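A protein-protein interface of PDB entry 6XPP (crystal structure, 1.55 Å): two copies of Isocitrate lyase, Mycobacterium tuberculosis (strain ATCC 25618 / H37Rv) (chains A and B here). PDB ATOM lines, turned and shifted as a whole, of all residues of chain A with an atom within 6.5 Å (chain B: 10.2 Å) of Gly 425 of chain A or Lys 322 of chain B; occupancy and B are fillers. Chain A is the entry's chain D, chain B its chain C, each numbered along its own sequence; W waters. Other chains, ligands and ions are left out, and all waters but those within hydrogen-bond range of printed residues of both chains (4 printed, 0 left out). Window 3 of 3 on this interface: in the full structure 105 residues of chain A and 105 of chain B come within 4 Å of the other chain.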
ATOM      1  N   GLU A 378     -12.991  26.889 -35.532  1.00  0.00           N
ATOM      2  CA  GLU A 378     -11.821  26.298 -36.237  1.00  0.00           C
ATOM      3  C   GLU A 378     -10.588  27.180 -36.011  1.00  0.00           C
ATOM      4  O   GLU A 378      -9.512  26.603 -35.803  1.00  0.00           O
ATOM      5  CB  GLU A 378     -12.162  26.029 -37.705  1.00  0.00           C
ATOM      6  CG  GLU A 378     -13.143  24.875 -37.865  1.00  0.00           C
ATOM      7  CD  GLU A 378     -12.604  23.527 -37.422  1.00  0.00           C
ATOM      8  OE1 GLU A 378     -11.476  23.198 -37.830  1.00  0.00           O
ATOM      9  OE2 GLU A 378     -13.299  22.816 -36.661  1.00  0.00           O
ATOM     10  N   LEU A 418     -17.198  17.413 -14.797  1.00  0.00           N
ATOM     11  CA  LEU A 418     -16.427  17.125 -16.045  1.00  0.00           C
ATOM     12  C   LEU A 418     -16.661  15.681 -16.508  1.00  0.00           C
ATOM     13  O   LEU A 418     -16.722  15.475 -17.739  1.00  0.00           O
ATOM     14  CB  LEU A 418     -14.938  17.429 -15.852  1.00  0.00           C
ATOM     15  CG  LEU A 418     -14.558  18.910 -15.933  1.00  0.00           C
ATOM     16  CD1 LEU A 418     -13.048  19.074 -15.826  1.00  0.00           C
ATOM     17  CD2 LEU A 418     -15.069  19.556 -17.218  1.00  0.00           C
ATOM     18  N   GLY A 420     -18.560  12.778 -17.853  1.00  0.00           N
ATOM     19  CA  GLY A 420     -19.803  12.692 -18.645  1.00  0.00           C
ATOM     20  C   GLY A 420     -20.081  13.968 -19.423  1.00  0.00           C
ATOM     21  O   GLY A 420     -21.118  14.014 -20.106  1.00  0.00           O
ATOM     22  N   SER A 421     -19.206  14.976 -19.333  1.00  0.00           N
ATOM     23  CA  SER A 421     -19.359  16.258 -20.067  1.00  0.00           C
ATOM     24  C   SER A 421     -19.080  16.026 -21.557  1.00  0.00           C
ATOM     25  O   SER A 421     -18.313  15.088 -21.887  1.00  0.00           O
ATOM     26  CB  SER A 421     -18.474  17.339 -19.494  1.00  0.00           C
ATOM     27  OG  SER A 421     -17.102  17.089 -19.773  1.00  0.00           O
ATOM     28  N   THR A 422     -19.652  16.856 -22.433  1.00  0.00           N
ATOM     29  CA  THR A 422     -19.346  16.819 -23.887  1.00  0.00           C
ATOM     30  C   THR A 422     -17.895  17.274 -24.099  1.00  0.00           C
ATOM     31  O   THR A 422     -17.291  16.866 -25.101  1.00  0.00           O
ATOM     32  CB  THR A 422     -20.355  17.640 -24.698  1.00  0.00           C
ATOM     33  OG1 THR A 422     -20.226  19.008 -24.321  1.00  0.00           O
ATOM     34  CG2 THR A 422     -21.780  17.184 -24.488  1.00  0.00           C
ATOM     35  N   GLU A 423     -17.337  18.073 -23.183  1.00  0.00           N
ATOM     36  CA  GLU A 423     -15.925  18.529 -23.276  1.00  0.00           C
ATOM     37  C   GLU A 423     -14.995  17.315 -23.162  1.00  0.00           C
ATOM     38  O   GLU A 423     -14.062  17.206 -23.980  1.00  0.00           O
ATOM     39  CB  GLU A 423     -15.606  19.555 -22.195  1.00  0.00           C
ATOM     40  CG  GLU A 423     -14.198  20.105 -22.306  1.00  0.00           C
ATOM     41  CD  GLU A 423     -13.987  21.436 -21.611  1.00  0.00           C
ATOM     42  OE1 GLU A 423     -14.550  22.446 -22.079  1.00  0.00           O
ATOM     43  OE2 GLU A 423     -13.293  21.439 -20.599  1.00  0.00           O
ATOM     44  N   GLU A 424     -15.253  16.446 -22.183  1.00  0.00           N
ATOM     45  CA  GLU A 424     -14.519  15.169 -21.973  1.00  0.00           C
ATOM     46  C   GLU A 424     -14.718  14.265 -23.202  1.00  0.00           C
ATOM     47  O   GLU A 424     -13.733  13.631 -23.631  1.00  0.00           O
ATOM     48  CB  GLU A 424     -15.004  14.514 -20.679  1.00  0.00           C
ATOM     49  CG  GLU A 424     -14.414  13.142 -20.411  1.00  0.00           C
ATOM     50  CD  GLU A 424     -14.961  12.475 -19.158  1.00  0.00           C
ATOM     51  OE1 GLU A 424     -16.090  11.931 -19.212  1.00  0.00           O
ATOM     52  OE2 GLU A 424     -14.270  12.521 -18.123  1.00  0.00           O
ATOM     53  N   GLY A 425     -15.931  14.236 -23.761  1.00  0.00           N
ATOM     54  CA  GLY A 425     -16.323  13.339 -24.866  1.00  0.00           C
ATOM     55  C   GLY A 425     -15.826  13.788 -26.237  1.00  0.00           C
ATOM     56  O   GLY A 425     -15.534  12.899 -27.054  1.00  0.00           O
ATOM     57  N   GLN A 426     -15.748  15.097 -26.515  1.00  0.00           N
ATOM     58  CA  GLN A 426     -15.626  15.636 -27.905  1.00  0.00           C
ATOM     59  C   GLN A 426     -14.400  16.542 -28.112  1.00  0.00           C
ATOM     60  O   GLN A 426     -14.151  16.914 -29.282  1.00  0.00           O
ATOM     61  CB  GLN A 426     -16.894  16.406 -28.274  1.00  0.00           C
ATOM     62  CG  GLN A 426     -18.160  15.556 -28.233  1.00  0.00           C
ATOM     63  CD  GLN A 426     -19.387  16.341 -28.641  1.00  0.00           C
ATOM     64  OE1 GLN A 426     -19.305  17.313 -29.393  1.00  0.00           O
ATOM     65  NE2 GLN A 426     -20.543  15.920 -28.151  1.00  0.00           N
ATOM     66  N   PHE A 427     -13.658  16.910 -27.060  1.00  0.00           N
ATOM     67  CA  PHE A 427     -12.544  17.899 -27.142  1.00  0.00           C
ATOM     68  C   PHE A 427     -11.218  17.262 -26.704  1.00  0.00           C
ATOM     69  O   PHE A 427     -11.150  16.081 -26.359  1.00  0.00           O
ATOM     70  CB  PHE A 427     -12.885  19.152 -26.326  1.00  0.00           C
ATOM     71  CG  PHE A 427     -13.940  20.027 -26.960  1.00  0.00           C
ATOM     72  CD1 PHE A 427     -15.271  19.631 -26.968  1.00  0.00           C
ATOM     73  CD2 PHE A 427     -13.600  21.222 -27.585  1.00  0.00           C
ATOM     74  CE1 PHE A 427     -16.237  20.421 -27.577  1.00  0.00           C
ATOM     75  CE2 PHE A 427     -14.571  22.012 -28.190  1.00  0.00           C
ATOM     76  CZ  PHE A 427     -15.888  21.611 -28.188  1.00  0.00           C
ATOM     77  N   HIS B 193     -24.374  20.600 -21.037  1.00  0.00           N
ATOM     78  CA  HIS B 193     -23.317  19.735 -21.627  1.00  0.00           C
ATOM     79  C   HIS B 193     -22.249  19.378 -20.588  1.00  0.00           C
ATOM     80  O   HIS B 193     -21.198  18.853 -20.997  1.00  0.00           O
ATOM     81  CB  HIS B 193     -22.782  20.408 -22.894  1.00  0.00           C
ATOM     82  CG  HIS B 193     -23.871  20.603 -23.894  1.00  0.00           C
ATOM     83  ND1 HIS B 193     -24.623  19.546 -24.374  1.00  0.00           N
ATOM     84  CD2 HIS B 193     -24.397  21.720 -24.442  1.00  0.00           C
ATOM     85  CE1 HIS B 193     -25.538  20.010 -25.201  1.00  0.00           C
ATOM     86  NE2 HIS B 193     -25.419  21.337 -25.265  1.00  0.00           N
ATOM     87  N   LEU B 194     -22.511  19.621 -19.298  1.00  0.00           N
ATOM     88  CA  LEU B 194     -21.692  19.066 -18.192  1.00  0.00           C
ATOM     89  C   LEU B 194     -22.378  17.802 -17.666  1.00  0.00           C
ATOM     90  O   LEU B 194     -23.591  17.624 -17.911  1.00  0.00           O
ATOM     91  CB  LEU B 194     -21.515  20.114 -17.086  1.00  0.00           C
ATOM     92  CG  LEU B 194     -20.502  21.220 -17.386  1.00  0.00           C
ATOM     93  CD1 LEU B 194     -20.493  22.272 -16.279  1.00  0.00           C
ATOM     94  CD2 LEU B 194     -19.104  20.643 -17.588  1.00  0.00           C
ATOM     95  N   GLY B 195     -21.606  16.935 -17.011  1.00  0.00           N
ATOM     96  CA  GLY B 195     -22.129  15.739 -16.335  1.00  0.00           C
ATOM     97  C   GLY B 195     -22.678  16.081 -14.963  1.00  0.00           C
ATOM     98  O   GLY B 195     -22.606  17.281 -14.566  1.00  0.00           O
ATOM     99  N   GLY B 287     -27.008  15.878 -26.870  1.00  0.00           N
ATOM    100  CA  GLY B 287     -25.586  15.499 -26.757  1.00  0.00           C
ATOM    101  C   GLY B 287     -24.795  15.810 -28.011  1.00  0.00           C
ATOM    102  O   GLY B 287     -23.566  15.937 -27.899  1.00  0.00           O
ATOM    103  N   THR B 288     -25.465  15.931 -29.161  1.00  0.00           N
ATOM    104  CA  THR B 288     -24.843  16.194 -30.485  1.00  0.00           C
ATOM    105  C   THR B 288     -25.770  17.074 -31.317  1.00  0.00           C
ATOM    106  O   THR B 288     -26.982  17.038 -31.149  1.00  0.00           O
ATOM    107  CB  THR B 288     -24.562  14.881 -31.225  1.00  0.00           C
ATOM    108  OG1 THR B 288     -25.821  14.253 -31.471  1.00  0.00           O
ATOM    109  CG2 THR B 288     -23.663  13.941 -30.452  1.00  0.00           C
ATOM    110  N   PRO B 289     -25.235  17.861 -32.275  1.00  0.00           N
ATOM    111  CA  PRO B 289     -26.071  18.615 -33.205  1.00  0.00           C
ATOM    112  C   PRO B 289     -26.575  17.663 -34.303  1.00  0.00           C
ATOM    113  O   PRO B 289     -25.844  17.393 -35.206  1.00  0.00           O
ATOM    114  CB  PRO B 289     -25.106  19.683 -33.727  1.00  0.00           C
ATOM    115  CG  PRO B 289     -23.745  19.002 -33.697  1.00  0.00           C
ATOM    116  CD  PRO B 289     -23.799  18.010 -32.554  1.00  0.00           C
ATOM    117  N   SER B 317     -20.383  23.882 -27.124  1.00  0.00           N
ATOM    118  CA  SER B 317     -19.968  22.663 -26.375  1.00  0.00           C
ATOM    119  C   SER B 317     -19.932  21.459 -27.318  1.00  0.00           C
ATOM    120  O   SER B 317     -19.401  20.408 -26.899  1.00  0.00           O
ATOM    121  CB  SER B 317     -20.855  22.395 -25.189  1.00  0.00           C
ATOM    122  OG  SER B 317     -20.688  23.380 -24.180  1.00  0.00           O
ATOM    123  N   PHE B 318     -20.473  21.601 -28.534  1.00  0.00           N
ATOM    124  CA  PHE B 318     -20.312  20.619 -29.638  1.00  0.00           C
ATOM    125  C   PHE B 318     -19.046  20.957 -30.417  1.00  0.00           C
ATOM    126  O   PHE B 318     -18.785  22.135 -30.671  1.00  0.00           O
ATOM    127  CB  PHE B 318     -21.495  20.620 -30.616  1.00  0.00           C
ATOM    128  CG  PHE B 318     -22.845  20.372 -29.991  1.00  0.00           C
ATOM    129  CD1 PHE B 318     -23.013  19.393 -29.022  1.00  0.00           C
ATOM    130  CD2 PHE B 318     -23.954  21.104 -30.396  1.00  0.00           C
ATOM    131  CE1 PHE B 318     -24.258  19.162 -28.461  1.00  0.00           C
ATOM    132  CE2 PHE B 318     -25.200  20.864 -29.841  1.00  0.00           C
ATOM    133  CZ  PHE B 318     -25.347  19.900 -28.873  1.00  0.00           C
ATOM    134  N   ASN B 319     -18.283  19.928 -30.789  1.00  0.00           N
ATOM    135  CA  ASN B 319     -17.194  20.034 -31.790  1.00  0.00           C
ATOM    136  C   ASN B 319     -17.852  19.853 -33.160  1.00  0.00           C
ATOM    137  O   ASN B 319     -18.125  18.689 -33.524  1.00  0.00           O
ATOM    138  CB  ASN B 319     -16.092  19.011 -31.503  1.00  0.00           C
ATOM    139  CG  ASN B 319     -14.912  19.133 -32.443  1.00  0.00           C
ATOM    140  OD1 ASN B 319     -15.047  19.631 -33.561  1.00  0.00           O
ATOM    141  ND2 ASN B 319     -13.755  18.671 -31.998  1.00  0.00           N
ATOM    142  N   TRP B 320     -18.147  20.953 -33.861  1.00  0.00           N
ATOM    143  CA  TRP B 320     -19.119  20.974 -34.990  1.00  0.00           C
ATOM    144  C   TRP B 320     -18.601  20.130 -36.157  1.00  0.00           C
ATOM    145  O   TRP B 320     -19.359  19.250 -36.612  1.00  0.00           O
ATOM    146  CB  TRP B 320     -19.470  22.410 -35.406  1.00  0.00           C
ATOM    147  CG  TRP B 320     -20.475  22.991 -34.462  1.00  0.00           C
ATOM    148  CD1 TRP B 320     -20.215  23.516 -33.234  1.00  0.00           C
ATOM    149  CD2 TRP B 320     -21.906  22.990 -34.608  1.00  0.00           C
ATOM    150  NE1 TRP B 320     -21.380  23.864 -32.614  1.00  0.00           N
ATOM    151  CE2 TRP B 320     -22.436  23.563 -33.433  1.00  0.00           C
ATOM    152  CE3 TRP B 320     -22.788  22.573 -35.611  1.00  0.00           C
ATOM    153  CZ2 TRP B 320     -23.806  23.732 -33.242  1.00  0.00           C
ATOM    154  CZ3 TRP B 320     -24.143  22.756 -35.427  1.00  0.00           C
ATOM    155  CH2 TRP B 320     -24.642  23.331 -34.258  1.00  0.00           C
ATOM    156  N   LYS B 321     -17.363  20.354 -36.600  1.00  0.00           N
ATOM    157  CA  LYS B 321     -16.815  19.674 -37.807  1.00  0.00           C
ATOM    158  C   LYS B 321     -16.406  18.229 -37.478  1.00  0.00           C
ATOM    159  O   LYS B 321     -16.184  17.461 -38.426  1.00  0.00           O
ATOM    160  CB  LYS B 321     -15.685  20.499 -38.425  1.00  0.00           C
ATOM    161  CG  LYS B 321     -16.177  21.638 -39.309  1.00  0.00           C
ATOM    162  CD  LYS B 321     -15.083  22.371 -40.059  1.00  0.00           C
ATOM    163  CE  LYS B 321     -14.400  21.527 -41.116  1.00  0.00           C
ATOM    164  NZ  LYS B 321     -15.374  20.903 -42.042  1.00  0.00           N
ATOM    165  N   LYS B 322     -16.356  17.845 -36.198  1.00  0.00           N
ATOM    166  CA  LYS B 322     -16.173  16.425 -35.787  1.00  0.00           C
ATOM    167  C   LYS B 322     -17.462  15.640 -36.074  1.00  0.00           C
ATOM    168  O   LYS B 322     -17.358  14.443 -36.371  1.00  0.00           O
ATOM    169  CB  LYS B 322     -15.776  16.321 -34.310  1.00  0.00           C
ATOM    170  CG  LYS B 322     -15.680  14.898 -33.771  1.00  0.00           C
ATOM    171  CD  LYS B 322     -15.054  14.788 -32.400  1.00  0.00           C
ATOM    172  CE  LYS B 322     -14.841  13.347 -31.982  1.00  0.00           C
ATOM    173  NZ  LYS B 322     -14.151  13.246 -30.678  1.00  0.00           N
ATOM    174  N   HIS B 323     -18.629  16.278 -35.973  1.00  0.00           N
ATOM    175  CA  HIS B 323     -19.957  15.625 -36.123  1.00  0.00           C
ATOM    176  C   HIS B 323     -20.523  15.821 -37.537  1.00  0.00           C
ATOM    177  O   HIS B 323     -21.152  14.872 -38.034  1.00  0.00           O
ATOM    178  CB  HIS B 323     -20.920  16.114 -35.028  1.00  0.00           C
ATOM    179  CG  HIS B 323     -20.536  15.636 -33.669  1.00  0.00           C
ATOM    180  ND1 HIS B 323     -20.730  14.324 -33.272  1.00  0.00           N
ATOM    181  CD2 HIS B 323     -19.945  16.266 -32.627  1.00  0.00           C
ATOM    182  CE1 HIS B 323     -20.289  14.173 -32.039  1.00  0.00           C
ATOM    183  NE2 HIS B 323     -19.793  15.348 -31.623  1.00  0.00           N
ATOM    184  N   LEU B 324     -20.332  16.989 -38.157  1.00  0.00           N
ATOM    185  CA  LEU B 324     -21.079  17.387 -39.384  1.00  0.00           C
ATOM    186  C   LEU B 324     -20.133  17.850 -40.490  1.00  0.00           C
ATOM    187  O   LEU B 324     -19.076  18.420 -40.175  1.00  0.00           O
ATOM    188  CB  LEU B 324     -22.056  18.515 -39.041  1.00  0.00           C
ATOM    189  CG  LEU B 324     -23.068  18.211 -37.941  1.00  0.00           C
ATOM    190  CD1 LEU B 324     -23.972  19.423 -37.734  1.00  0.00           C
ATOM    191  CD2 LEU B 324     -23.911  16.985 -38.289  1.00  0.00           C
ATOM    192  N   ASP B 325     -20.551  17.651 -41.746  1.00  0.00           N
ATOM    193  CA  ASP B 325     -19.880  18.210 -42.949  1.00  0.00           C
ATOM    194  C   ASP B 325     -20.353  19.652 -43.157  1.00  0.00           C
ATOM    195  O   ASP B 325     -21.367  20.058 -42.537  1.00  0.00           O
ATOM    196  CB  ASP B 325     -20.103  17.340 -44.193  1.00  0.00           C
ATOM    197  CG  ASP B 325     -21.544  17.159 -44.642  1.00  0.00           C
ATOM    198  OD1 ASP B 325     -22.374  18.053 -44.380  1.00  0.00           O
ATOM    199  OD2 ASP B 325     -21.827  16.116 -45.272  1.00  0.00           O
ATOM    200  N   ASP B 326     -19.649  20.391 -44.013  1.00  0.00           N
ATOM    201  CA  ASP B 326     -19.874  21.841 -44.245  1.00  0.00           C
ATOM    202  C   ASP B 326     -21.282  22.071 -44.807  1.00  0.00           C
ATOM    203  O   ASP B 326     -21.901  23.081 -44.432  1.00  0.00           O
ATOM    204  CB  ASP B 326     -18.776  22.429 -45.136  1.00  0.00           C
ATOM    205  CG  ASP B 326     -17.464  22.665 -44.407  1.00  0.00           C
ATOM    206  OD1 ASP B 326     -17.433  22.505 -43.176  1.00  0.00           O
ATOM    207  OD2 ASP B 326     -16.480  23.021 -45.073  1.00  0.00           O
ATOM    208  N   ILE B 329     -23.783  21.818 -41.888  1.00  0.00           N
ATOM    209  CA  ILE B 329     -23.550  23.034 -41.050  1.00  0.00           C
ATOM    210  C   ILE B 329     -24.234  24.235 -41.717  1.00  0.00           C
ATOM    211  O   ILE B 329     -24.914  24.994 -41.002  1.00  0.00           O
ATOM    212  CB  ILE B 329     -22.042  23.257 -40.822  1.00  0.00           C
ATOM    213  CG1 ILE B 329     -21.454  22.161 -39.929  1.00  0.00           C
ATOM    214  CG2 ILE B 329     -21.777  24.651 -40.263  1.00  0.00           C
ATOM    215  CD1 ILE B 329     -19.946  22.086 -39.947  1.00  0.00           C
HETATM  216  O   HOH W   1     -13.372  20.068 -35.450  1.00  0.00           O
HETATM  217  O   HOH W   2     -15.838  22.612 -35.709  1.00  0.00           O
HETATM  218  O   HOH W   3     -19.062  20.452 -22.102  1.00  0.00           O
HETATM  219  O   HOH W   4     -17.935  20.932 -24.531  1.00  0.00           O
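Lys 321 of chain B touches Glu 378 of chain A. His 193 of chain B touches Ser 421 of chain A (O to CA, 3.3 Å). CD2 of Leu 194 of chain B touches CB of Ser 421 of chain A, at 3.9 Å. Ser 421 of chain A touches Gly 195 of chain B. Ser 317 of chain B touches Gln 426 of chain A (O to OE1, 3.98 Å). Phe 318 of chain B touches Gln 426 of chain A (CA to OE1, 3.5 Å). Lys 322 of chain B touches Gln 426 of chain A. Ser 317 of chain B touches Phe 427 of chain A (O to CE1, 3.2 Å). CZ of Phe 427 of chain A touches O of Phe 318 of chain B (3.9 Å). Phe 427 of chain A touches Asn 319 of chain B (CE1 to N, 3.8 Å).
Of the 10 printed residues of chain A, 6 touch a printed residue of chain B. Hydrophobic or aromatic side chains of chain A that line the printed part of chain B: Phe 427. Of the 17 printed residues of chain B, 10 touch a printed residue of chain A. Printed residues of chain B that touch a printed residue of chain A: His 193, Leu 194, Gly 195, Gly 287, Ser 317, Phe 318, Asn 319, Lys 321, Lys 322 and His 323. Hydrophobic or aromatic side chains of chain B that line the printed part of chain A: His 193, Leu 194 and His 323. Along chain B the printed residues that touch a printed residue of chain A span positions 193 to 323.
N of Thr 422 of chain A is in hydrogen-bond range of O of His 193 of chain B (2.9 Å). O of Gly 287 of chain B lies within hydrogen-bond range of NE2 of Gln 426 of chain A (3.0 Å). O of Ser 317 of chain B lies within hydrogen-bond range of OG1 of Thr 422 of chain A (3.0 Å). N of Asn 319 of chain B lies within hydrogen-bond range of OE1 of Gln 426 of chain A (3.1 Å). A ring nitrogen (NE2) of His 323 of chain B sits at hydrogen-bond distance from the side-chain amide oxygen of Gln 426 of chain A, at 3.0 Å.
The side-chain amide oxygen (OD1) of Asn 319 of chain B is in hydrogen-bond range of the backbone NH (N) of Lys 322 of chain B, at 3.4 Å. NZ of Lys 321 of chain B lies within salt-bridge range of OD1 of Asp 326 of chain B, 2.8 Å away. The backbone carbonyl oxygen of Leu 418 of chain A lies within hydrogen-bond range of the side-chain hydroxyl of Ser 421 of chain A (2.6 Å). The backbone NH (N) of Glu 424 of chain A is in hydrogen-bond range of the side-chain hydroxyl (OG) of Ser 421 of chain A (3.1 Å).
Gly 425 of chain A touches just one residue of chain B: Lys 322. Lys 322 of chain B touches just these residues of chain A: Gly 425 and Gln 426. Of chain B, only His 193 (3.3 Å), Leu 194 (3.9 Å) and Gly 195 (3.9 Å) come within 4 Å of Ser 421 of chain A. No residue of chain B comes within 4 Å of Glu 424 of chain A. Printed residues of chain B within 4 Å of Gln 426 of chain A: Gly 287, Ser 317, Phe 318, Asn 319, Lys 322 and His 323. Printed residues of chain B within 4 Å of Thr 422 of chain A: His 193 (2.9 Å) and Ser 317 (3.0 Å). Of the printed residues of chain A, Gly 195 of chain B touches Ser 421. Of the printed residues of chain B, Glu 378 of chain A touches Lys 321 (3.8 Å). Of the printed residues of chain A, Asn 319 of chain B touches Gln 426 (3.1 Å) and Phe 427 (3.8 Å). Of the printed residues of chain A, Leu 194 of chain B touches Ser 421. Ile 329 of chain B touches none of the printed residues of chain A. Asp 325 of chain B touches none of the printed residues of chain A. The nearest residue of chain B that does not touch Gly 425 of chain A is His 323 of chain B (6.7 Å). The nearest printed residue of chain A that does not touch Phe 318 of chain B is Thr 422 of chain A (5.0 Å).
Water W1 lies within hydrogen-bond range of OD1 of Asn 319 of chain B (2.6 Å) and OE2 of Glu 378 of chain A (3.0 Å). Water W2 lies within hydrogen-bond range of the side-chain carboxylate (OE2) of Glu 378 of chain A (2.7 Å), the backbone NH (N) of Lys 321 of chain B (2.9 Å) and the backbone NH (N) of Trp 320 of chain B (3.4 Å). Water W4 lies within hydrogen-bond range of the backbone carbonyl oxygen (O) of Ser 317 of chain B (2.8 Å), the side-chain hydroxyl (OG1) of Thr 422 of chain A (3.0 Å) and the backbone NH (N) of Glu 423 of chain A (3.2 Å). Water W3 lies within hydrogen-bond range of the backbone carbonyl oxygen of His 193 of chain B, the side-chain hydroxyl of Thr 422 of chain A and the backbone NH of Glu 423 of chain A.
No position is printed for both chains. Of the 16 pairs that touch across the chains among the printed residues, none has its exchanged pair printed and touching as well.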
